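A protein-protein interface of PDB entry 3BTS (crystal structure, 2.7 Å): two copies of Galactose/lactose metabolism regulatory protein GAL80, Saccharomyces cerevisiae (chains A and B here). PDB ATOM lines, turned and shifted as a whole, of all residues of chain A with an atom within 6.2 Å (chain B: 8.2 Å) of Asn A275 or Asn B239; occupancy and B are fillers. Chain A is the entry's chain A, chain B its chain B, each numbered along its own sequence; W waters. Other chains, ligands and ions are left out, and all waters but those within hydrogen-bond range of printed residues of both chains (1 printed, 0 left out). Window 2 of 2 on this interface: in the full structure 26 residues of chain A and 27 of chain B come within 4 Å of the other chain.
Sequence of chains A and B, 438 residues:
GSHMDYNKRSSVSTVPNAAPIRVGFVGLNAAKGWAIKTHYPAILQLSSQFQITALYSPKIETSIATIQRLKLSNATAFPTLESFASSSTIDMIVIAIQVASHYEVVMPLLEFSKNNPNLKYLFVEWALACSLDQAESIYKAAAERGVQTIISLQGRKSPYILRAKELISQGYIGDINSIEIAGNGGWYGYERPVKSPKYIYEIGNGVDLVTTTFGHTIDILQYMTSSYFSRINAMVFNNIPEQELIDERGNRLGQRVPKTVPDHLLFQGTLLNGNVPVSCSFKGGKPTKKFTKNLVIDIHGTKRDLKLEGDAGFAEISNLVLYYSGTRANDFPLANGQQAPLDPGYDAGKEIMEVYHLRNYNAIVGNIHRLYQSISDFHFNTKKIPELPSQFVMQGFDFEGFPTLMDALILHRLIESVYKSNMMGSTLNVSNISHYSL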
ATOM      1  N   ASN A 177      16.637  36.653  26.721  1.00  0.00           N
ATOM      2  CA  ASN A 177      17.556  35.825  27.479  1.00  0.00           C
ATOM      3  C   ASN A 177      16.817  34.730  28.252  1.00  0.00           C
ATOM      4  O   ASN A 177      17.265  33.587  28.305  1.00  0.00           O
ATOM      5  CB  ASN A 177      18.392  36.698  28.433  1.00  0.00           C
ATOM      6  CG  ASN A 177      19.179  35.878  29.438  1.00  0.00           C
ATOM      7  OD1 ASN A 177      18.724  35.645  30.557  1.00  0.00           O
ATOM      8  ND2 ASN A 177      20.357  35.415  29.034  1.00  0.00           N
ATOM      9  N   SER A 230      10.259  24.075  21.351  1.00  0.00           N
ATOM     10  CA  SER A 230      10.864  22.871  20.808  1.00  0.00           C
ATOM     11  C   SER A 230      10.801  21.727  21.812  1.00  0.00           C
ATOM     12  O   SER A 230      10.342  20.632  21.483  1.00  0.00           O
ATOM     13  CB  SER A 230      12.295  23.119  20.332  1.00  0.00           C
ATOM     14  OG  SER A 230      13.104  23.621  21.364  1.00  0.00           O
ATOM     15  N   THR A 270      11.579  25.385  26.053  1.00  0.00           N
ATOM     16  CA  THR A 270      12.437  26.253  25.269  1.00  0.00           C
ATOM     17  C   THR A 270      11.705  26.724  24.039  1.00  0.00           C
ATOM     18  O   THR A 270      10.995  25.957  23.394  1.00  0.00           O
ATOM     19  CB  THR A 270      13.725  25.540  24.826  1.00  0.00           C
ATOM     20  OG1 THR A 270      13.413  24.224  24.369  1.00  0.00           O
ATOM     21  CG2 THR A 270      14.701  25.443  25.976  1.00  0.00           C
ATOM     22  N   LEU A 271      11.884  27.996  23.718  1.00  0.00           N
ATOM     23  CA  LEU A 271      11.330  28.543  22.493  1.00  0.00           C
ATOM     24  C   LEU A 271      12.255  28.195  21.341  1.00  0.00           C
ATOM     25  O   LEU A 271      13.465  28.193  21.510  1.00  0.00           O
ATOM     26  CB  LEU A 271      11.178  30.056  22.614  1.00  0.00           C
ATOM     27  CG  LEU A 271      10.152  30.540  23.641  1.00  0.00           C
ATOM     28  CD1 LEU A 271      10.001  32.032  23.503  1.00  0.00           C
ATOM     29  CD2 LEU A 271       8.805  29.832  23.458  1.00  0.00           C
ATOM     30  N   LEU A 272      11.687  27.875  20.183  1.00  0.00           N
ATOM     31  CA  LEU A 272      12.481  27.583  18.989  1.00  0.00           C
ATOM     32  C   LEU A 272      13.409  28.745  18.640  1.00  0.00           C
ATOM     33  O   LEU A 272      14.624  28.574  18.528  1.00  0.00           O
ATOM     34  CB  LEU A 272      11.567  27.284  17.799  1.00  0.00           C
ATOM     35  CG  LEU A 272      10.977  25.878  17.751  1.00  0.00           C
ATOM     36  CD1 LEU A 272       9.759  25.820  16.842  1.00  0.00           C
ATOM     37  CD2 LEU A 272      12.046  24.917  17.295  1.00  0.00           C
ATOM     38  N   ASN A 273      12.824  29.926  18.460  1.00  0.00           N
ATOM     39  CA  ASN A 273      13.603  31.116  18.174  1.00  0.00           C
ATOM     40  C   ASN A 273      14.488  31.484  19.359  1.00  0.00           C
ATOM     41  O   ASN A 273      14.012  32.028  20.353  1.00  0.00           O
ATOM     42  CB  ASN A 273      12.696  32.293  17.790  1.00  0.00           C
ATOM     43  CG  ASN A 273      11.916  32.042  16.504  1.00  0.00           C
ATOM     44  OD1 ASN A 273      11.992  30.961  15.912  1.00  0.00           O
ATOM     45  ND2 ASN A 273      11.159  33.045  16.069  1.00  0.00           N
ATOM     46  N   GLY A 274      15.775  31.163  19.252  1.00  0.00           N
ATOM     47  CA  GLY A 274      16.758  31.581  20.237  1.00  0.00           C
ATOM     48  C   GLY A 274      16.968  30.579  21.356  1.00  0.00           C
ATOM     49  O   GLY A 274      17.793  30.791  22.245  1.00  0.00           O
ATOM     50  N   ASN A 275      16.222  29.482  21.317  1.00  0.00           N
ATOM     51  CA  ASN A 275      16.294  28.477  22.374  1.00  0.00           C
ATOM     52  C   ASN A 275      16.140  29.088  23.775  1.00  0.00           C
ATOM     53  O   ASN A 275      16.868  28.741  24.713  1.00  0.00           O
ATOM     54  CB  ASN A 275      17.600  27.693  22.273  1.00  0.00           C
ATOM     55  CG  ASN A 275      17.539  26.375  22.999  1.00  0.00           C
ATOM     56  OD1 ASN A 275      16.577  25.620  22.857  1.00  0.00           O
ATOM     57  ND2 ASN A 275      18.568  26.087  23.783  1.00  0.00           N
ATOM     58  N   VAL A 276      15.186  30.005  23.903  1.00  0.00           N
ATOM     59  CA  VAL A 276      14.935  30.713  25.151  1.00  0.00           C
ATOM     60  C   VAL A 276      14.307  29.835  26.238  1.00  0.00           C
ATOM     61  O   VAL A 276      13.304  29.154  26.006  1.00  0.00           O
ATOM     62  CB  VAL A 276      14.021  31.915  24.902  1.00  0.00           C
ATOM     63  CG1 VAL A 276      13.774  32.683  26.198  1.00  0.00           C
ATOM     64  CG2 VAL A 276      14.628  32.801  23.843  1.00  0.00           C
ATOM     65  N   PRO A 277      14.903  29.852  27.435  1.00  0.00           N
ATOM     66  CA  PRO A 277      14.423  29.139  28.627  1.00  0.00           C
ATOM     67  C   PRO A 277      13.157  29.777  29.184  1.00  0.00           C
ATOM     68  O   PRO A 277      13.105  30.997  29.325  1.00  0.00           O
ATOM     69  CB  PRO A 277      15.566  29.317  29.638  1.00  0.00           C
ATOM     70  CG  PRO A 277      16.737  29.744  28.840  1.00  0.00           C
ATOM     71  CD  PRO A 277      16.182  30.529  27.687  1.00  0.00           C
ATOM     72  N   TYR B 188      28.519  34.252  34.852  1.00  0.00           N
ATOM     73  CA  TYR B 188      28.086  33.366  33.783  1.00  0.00           C
ATOM     74  C   TYR B 188      27.081  34.051  32.864  1.00  0.00           C
ATOM     75  O   TYR B 188      26.295  33.396  32.183  1.00  0.00           O
ATOM     76  CB  TYR B 188      27.552  32.052  34.353  1.00  0.00           C
ATOM     77  CG  TYR B 188      28.516  31.410  35.327  1.00  0.00           C
ATOM     78  CD1 TYR B 188      29.807  31.082  34.936  1.00  0.00           C
ATOM     79  CD2 TYR B 188      28.144  31.148  36.641  1.00  0.00           C
ATOM     80  CE1 TYR B 188      30.697  30.505  35.821  1.00  0.00           C
ATOM     81  CE2 TYR B 188      29.026  30.566  37.533  1.00  0.00           C
ATOM     82  CZ  TYR B 188      30.303  30.247  37.115  1.00  0.00           C
ATOM     83  OH  TYR B 188      31.198  29.673  37.989  1.00  0.00           O
ATOM     84  N   GLY B 189      27.129  35.381  32.849  1.00  0.00           N
ATOM     85  CA  GLY B 189      26.339  36.161  31.917  1.00  0.00           C
ATOM     86  C   GLY B 189      27.092  36.342  30.612  1.00  0.00           C
ATOM     87  O   GLY B 189      27.917  35.506  30.232  1.00  0.00           O
ATOM     88  N   TYR B 190      26.826  37.443  29.922  1.00  0.00           N
ATOM     89  CA  TYR B 190      27.437  37.664  28.618  1.00  0.00           C
ATOM     90  C   TYR B 190      28.881  38.148  28.735  1.00  0.00           C
ATOM     91  O   TYR B 190      29.580  38.284  27.733  1.00  0.00           O
ATOM     92  CB  TYR B 190      26.617  38.660  27.793  1.00  0.00           C
ATOM     93  CG  TYR B 190      25.268  38.146  27.311  1.00  0.00           C
ATOM     94  CD1 TYR B 190      24.116  38.910  27.460  1.00  0.00           C
ATOM     95  CD2 TYR B 190      25.150  36.901  26.700  1.00  0.00           C
ATOM     96  CE1 TYR B 190      22.886  38.453  27.015  1.00  0.00           C
ATOM     97  CE2 TYR B 190      23.925  36.435  26.253  1.00  0.00           C
ATOM     98  CZ  TYR B 190      22.794  37.215  26.414  1.00  0.00           C
ATOM     99  OH  TYR B 190      21.570  36.756  25.973  1.00  0.00           O
ATOM    100  N   MET B 235      16.569  21.273  32.985  1.00  0.00           N
ATOM    101  CA  MET B 235      17.165  21.584  31.701  1.00  0.00           C
ATOM    102  C   MET B 235      18.318  22.537  31.973  1.00  0.00           C
ATOM    103  O   MET B 235      18.140  23.547  32.648  1.00  0.00           O
ATOM    104  CB  MET B 235      16.137  22.204  30.751  1.00  0.00           C
ATOM    105  CG  MET B 235      14.935  21.315  30.500  1.00  0.00           C
ATOM    106  SD  MET B 235      13.661  22.077  29.476  1.00  0.00           S
ATOM    107  CE  MET B 235      12.313  20.920  29.706  1.00  0.00           C
ATOM    108  N   VAL B 236      19.499  22.192  31.464  1.00  0.00           N
ATOM    109  CA  VAL B 236      20.719  22.972  31.654  1.00  0.00           C
ATOM    110  C   VAL B 236      21.172  23.562  30.322  1.00  0.00           C
ATOM    111  O   VAL B 236      21.170  22.862  29.314  1.00  0.00           O
ATOM    112  CB  VAL B 236      21.855  22.080  32.200  1.00  0.00           C
ATOM    113  CG1 VAL B 236      23.161  22.873  32.333  1.00  0.00           C
ATOM    114  CG2 VAL B 236      21.453  21.459  33.524  1.00  0.00           C
ATOM    115  N   PHE B 237      21.578  24.832  30.325  1.00  0.00           N
ATOM    116  CA  PHE B 237      21.885  25.556  29.082  1.00  0.00           C
ATOM    117  C   PHE B 237      23.311  26.104  28.975  1.00  0.00           C
ATOM    118  O   PHE B 237      23.886  26.566  29.958  1.00  0.00           O
ATOM    119  CB  PHE B 237      20.924  26.739  28.913  1.00  0.00           C
ATOM    120  CG  PHE B 237      19.477  26.346  28.868  1.00  0.00           C
ATOM    121  CD1 PHE B 237      18.833  25.881  30.007  1.00  0.00           C
ATOM    122  CD2 PHE B 237      18.756  26.447  27.690  1.00  0.00           C
ATOM    123  CE1 PHE B 237      17.506  25.507  29.968  1.00  0.00           C
ATOM    124  CE2 PHE B 237      17.424  26.078  27.644  1.00  0.00           C
ATOM    125  CZ  PHE B 237      16.796  25.609  28.785  1.00  0.00           C
ATOM    126  N   ASN B 238      23.866  26.068  27.769  1.00  0.00           N
ATOM    127  CA  ASN B 238      25.042  26.875  27.453  1.00  0.00           C
ATOM    128  C   ASN B 238      24.785  27.718  26.206  1.00  0.00           C
ATOM    129  O   ASN B 238      25.409  27.522  25.162  1.00  0.00           O
ATOM    130  CB  ASN B 238      26.306  26.022  27.284  1.00  0.00           C
ATOM    131  CG  ASN B 238      27.563  26.872  27.133  1.00  0.00           C
ATOM    132  OD1 ASN B 238      27.525  28.095  27.290  1.00  0.00           O
ATOM    133  ND2 ASN B 238      28.683  26.228  26.827  1.00  0.00           N
ATOM    134  N   ASN B 239      23.851  28.655  26.331  1.00  0.00           N
ATOM    135  CA  ASN B 239      23.462  29.524  25.230  1.00  0.00           C
ATOM    136  C   ASN B 239      24.476  30.623  24.993  1.00  0.00           C
ATOM    137  O   ASN B 239      24.386  31.355  24.005  1.00  0.00           O
ATOM    138  CB  ASN B 239      22.094  30.150  25.511  1.00  0.00           C
ATOM    139  CG  ASN B 239      20.959  29.144  25.414  1.00  0.00           C
ATOM    140  OD1 ASN B 239      21.159  27.997  25.007  1.00  0.00           O
ATOM    141  ND2 ASN B 239      19.759  29.575  25.783  1.00  0.00           N
ATOM    142  N   ILE B 240      25.432  30.734  25.916  1.00  0.00           N
ATOM    143  CA  ILE B 240      26.511  31.708  25.833  1.00  0.00           C
ATOM    144  C   ILE B 240      27.867  30.993  25.876  1.00  0.00           C
ATOM    145  O   ILE B 240      28.544  30.998  26.904  1.00  0.00           O
ATOM    146  CB  ILE B 240      26.424  32.715  27.000  1.00  0.00           C
ATOM    147  CG1 ILE B 240      24.993  33.237  27.150  1.00  0.00           C
ATOM    148  CG2 ILE B 240      27.410  33.868  26.824  1.00  0.00           C
ATOM    149  CD1 ILE B 240      24.739  33.965  28.469  1.00  0.00           C
ATOM    150  N   PRO B 241      28.263  30.375  24.751  1.00  0.00           N
ATOM    151  CA  PRO B 241      29.506  29.601  24.647  1.00  0.00           C
ATOM    152  C   PRO B 241      30.742  30.493  24.609  1.00  0.00           C
ATOM    153  O   PRO B 241      31.836  30.048  24.964  1.00  0.00           O
ATOM    154  CB  PRO B 241      29.359  28.875  23.305  1.00  0.00           C
ATOM    155  CG  PRO B 241      27.923  29.063  22.896  1.00  0.00           C
ATOM    156  CD  PRO B 241      27.510  30.360  23.489  1.00  0.00           C
ATOM    157  N   GLU B 242      30.557  31.735  24.171  1.00  0.00           N
ATOM    158  CA  GLU B 242      31.631  32.723  24.143  1.00  0.00           C
ATOM    159  C   GLU B 242      31.267  33.930  25.010  1.00  0.00           C
ATOM    160  O   GLU B 242      30.173  34.483  24.891  1.00  0.00           O
ATOM    161  CB  GLU B 242      31.904  33.166  22.702  1.00  0.00           C
ATOM    162  CG  GLU B 242      32.320  32.033  21.766  1.00  0.00           C
ATOM    163  CD  GLU B 242      33.718  31.514  22.063  1.00  0.00           C
ATOM    164  OE1 GLU B 242      34.617  32.339  22.349  1.00  0.00           O
ATOM    165  OE2 GLU B 242      33.915  30.282  22.012  1.00  0.00           O
ATOM    166  N   LYS B 259      33.387  29.343  27.115  1.00  0.00           N
ATOM    167  CA  LYS B 259      32.857  28.960  28.403  1.00  0.00           C
ATOM    168  C   LYS B 259      32.018  27.707  28.224  1.00  0.00           C
ATOM    169  O   LYS B 259      31.018  27.728  27.514  1.00  0.00           O
ATOM    170  CB  LYS B 259      32.012  30.097  28.961  1.00  0.00           C
ATOM    171  CG  LYS B 259      30.863  29.648  29.835  1.00  0.00           C
ATOM    172  CD  LYS B 259      30.160  30.848  30.450  1.00  0.00           C
ATOM    173  CE  LYS B 259      28.675  30.574  30.639  1.00  0.00           C
ATOM    174  NZ  LYS B 259      28.073  29.918  29.439  1.00  0.00           N
ATOM    175  N   VAL B 261      30.886  25.878  30.998  1.00  0.00           N
ATOM    176  CA  VAL B 261      29.940  25.807  32.115  1.00  0.00           C
ATOM    177  C   VAL B 261      28.641  26.519  31.749  1.00  0.00           C
ATOM    178  O   VAL B 261      28.633  27.391  30.884  1.00  0.00           O
ATOM    179  CB  VAL B 261      30.520  26.375  33.445  1.00  0.00           C
ATOM    180  CG1 VAL B 261      31.661  25.499  33.949  1.00  0.00           C
ATOM    181  CG2 VAL B 261      30.963  27.821  33.285  1.00  0.00           C
ATOM    182  N   PRO B 262      27.535  26.143  32.408  1.00  0.00           N
ATOM    183  CA  PRO B 262      26.180  26.588  32.044  1.00  0.00           C
ATOM    184  C   PRO B 262      25.873  28.052  32.382  1.00  0.00           C
ATOM    185  O   PRO B 262      26.403  28.601  33.352  1.00  0.00           O
ATOM    186  CB  PRO B 262      25.267  25.664  32.867  1.00  0.00           C
ATOM    187  CG  PRO B 262      26.167  24.621  33.475  1.00  0.00           C
ATOM    188  CD  PRO B 262      27.519  25.235  33.565  1.00  0.00           C
ATOM    189  N   ASP B 263      25.002  28.662  31.579  1.00  0.00           N
ATOM    190  CA  ASP B 263      24.552  30.040  31.796  1.00  0.00           C
ATOM    191  C   ASP B 263      23.076  30.131  32.227  1.00  0.00           C
ATOM    192  O   ASP B 263      22.586  31.207  32.582  1.00  0.00           O
ATOM    193  CB  ASP B 263      24.798  30.899  30.549  1.00  0.00           C
ATOM    194  CG  ASP B 263      24.565  30.134  29.259  1.00  0.00           C
ATOM    195  OD1 ASP B 263      23.386  29.924  28.894  1.00  0.00           O
ATOM    196  OD2 ASP B 263      25.563  29.744  28.612  1.00  0.00           O
ATOM    197  N   HIS B 264      22.381  28.996  32.195  1.00  0.00           N
ATOM    198  CA  HIS B 264      20.991  28.926  32.639  1.00  0.00           C
ATOM    199  C   HIS B 264      20.643  27.540  33.173  1.00  0.00           C
ATOM    200  O   HIS B 264      21.100  26.529  32.645  1.00  0.00           O
ATOM    201  CB  HIS B 264      20.032  29.291  31.501  1.00  0.00           C
ATOM    202  CG  HIS B 264      20.241  30.667  30.944  1.00  0.00           C
ATOM    203  ND1 HIS B 264      19.642  31.786  31.479  1.00  0.00           N
ATOM    204  CD2 HIS B 264      20.979  31.099  29.890  1.00  0.00           C
ATOM    205  CE1 HIS B 264      20.008  32.852  30.786  1.00  0.00           C
ATOM    206  NE2 HIS B 264      20.816  32.460  29.816  1.00  0.00           N
ATOM    207  N   LEU B 266      17.029  25.497  34.389  1.00  0.00           N
ATOM    208  CA  LEU B 266      15.614  25.355  34.729  1.00  0.00           C
ATOM    209  C   LEU B 266      15.451  24.118  35.595  1.00  0.00           C
ATOM    210  O   LEU B 266      15.979  23.049  35.275  1.00  0.00           O
ATOM    211  CB  LEU B 266      14.757  25.199  33.479  1.00  0.00           C
ATOM    212  CG  LEU B 266      14.685  26.384  32.522  1.00  0.00           C
ATOM    213  CD1 LEU B 266      13.810  26.035  31.335  1.00  0.00           C
ATOM    214  CD2 LEU B 266      14.140  27.591  33.233  1.00  0.00           C
HETATM  215  O   HOH W   1      19.266  32.485  26.715  1.00  0.00           O
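Asn A275 touches just these residues of chain B: Phe B237 (3.9 Å) and Asn B239 (3.2 Å). Of the printed residues of chain B, Pro A277 touches Phe B237. Of the printed residues of chain A, Tyr B190 touches Asn A177. Of the printed residues of chain A, Asn B239 touches Asn A275 (3.2 Å). Val B261 touches none of the printed residues of chain A. The nearest residue of chain B that does not touch Asn A275 is Asn B238 (6.6 Å).
Among the printed residues, merely in contact across the chains: Thr A270 with Phe B237 (3.3 Å), Asn A177 with Tyr B190 (3.6 Å), Pro A277 with Phe B237 (3.9 Å) and Asn A275 with Phe B237 (3.9 Å).
No position is printed for both chains.
OD1 of Asp B263 is in hydrogen-bond range of N of Asn B239, at 2.9 Å. The backbone carbonyl oxygen of His B264 is in hydrogen-bond range of the backbone NH of Phe B237 (2.9 Å). The backbone NH (N) of Asp B263 is in hydrogen-bond range of the backbone carbonyl oxygen (O) of Phe B237, at 2.9 Å. The backbone carbonyl oxygen of Thr A270 sits at hydrogen-bond distance from the backbone NH of Ser A230 (2.9 Å).
Water W1 lies within hydrogen-bond range of O of Asn A177 (2.8 Å), ND2 of Asn B239 (3.1 Å) and NE2 of His B264 (3.5 Å).
Printed residues of chain A that touch a printed residue of chain B: Asn A177, Thr A270, Asn A275 and Pro A277. Of the 17 printed residues of chain B, 4 touch a printed residue of chain A. Hydrophobic or aromatic side chains of chain B that line the printed part of chain A: Tyr B190, Phe B237 and His B264. Among the printed residues, 6 pairs touch across the chains. Among the printed residues, no Asp or Glu carboxylate lies within 4 Å of a Lys or Arg side-chain nitrogen of the other chain.
NE2 of His B264 sits at hydrogen-bond distance from ND2 of Asn A177 (3.1 Å). O of Asn A275 is in hydrogen-bond range of ND2 of Asn B239 (3.2 Å).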
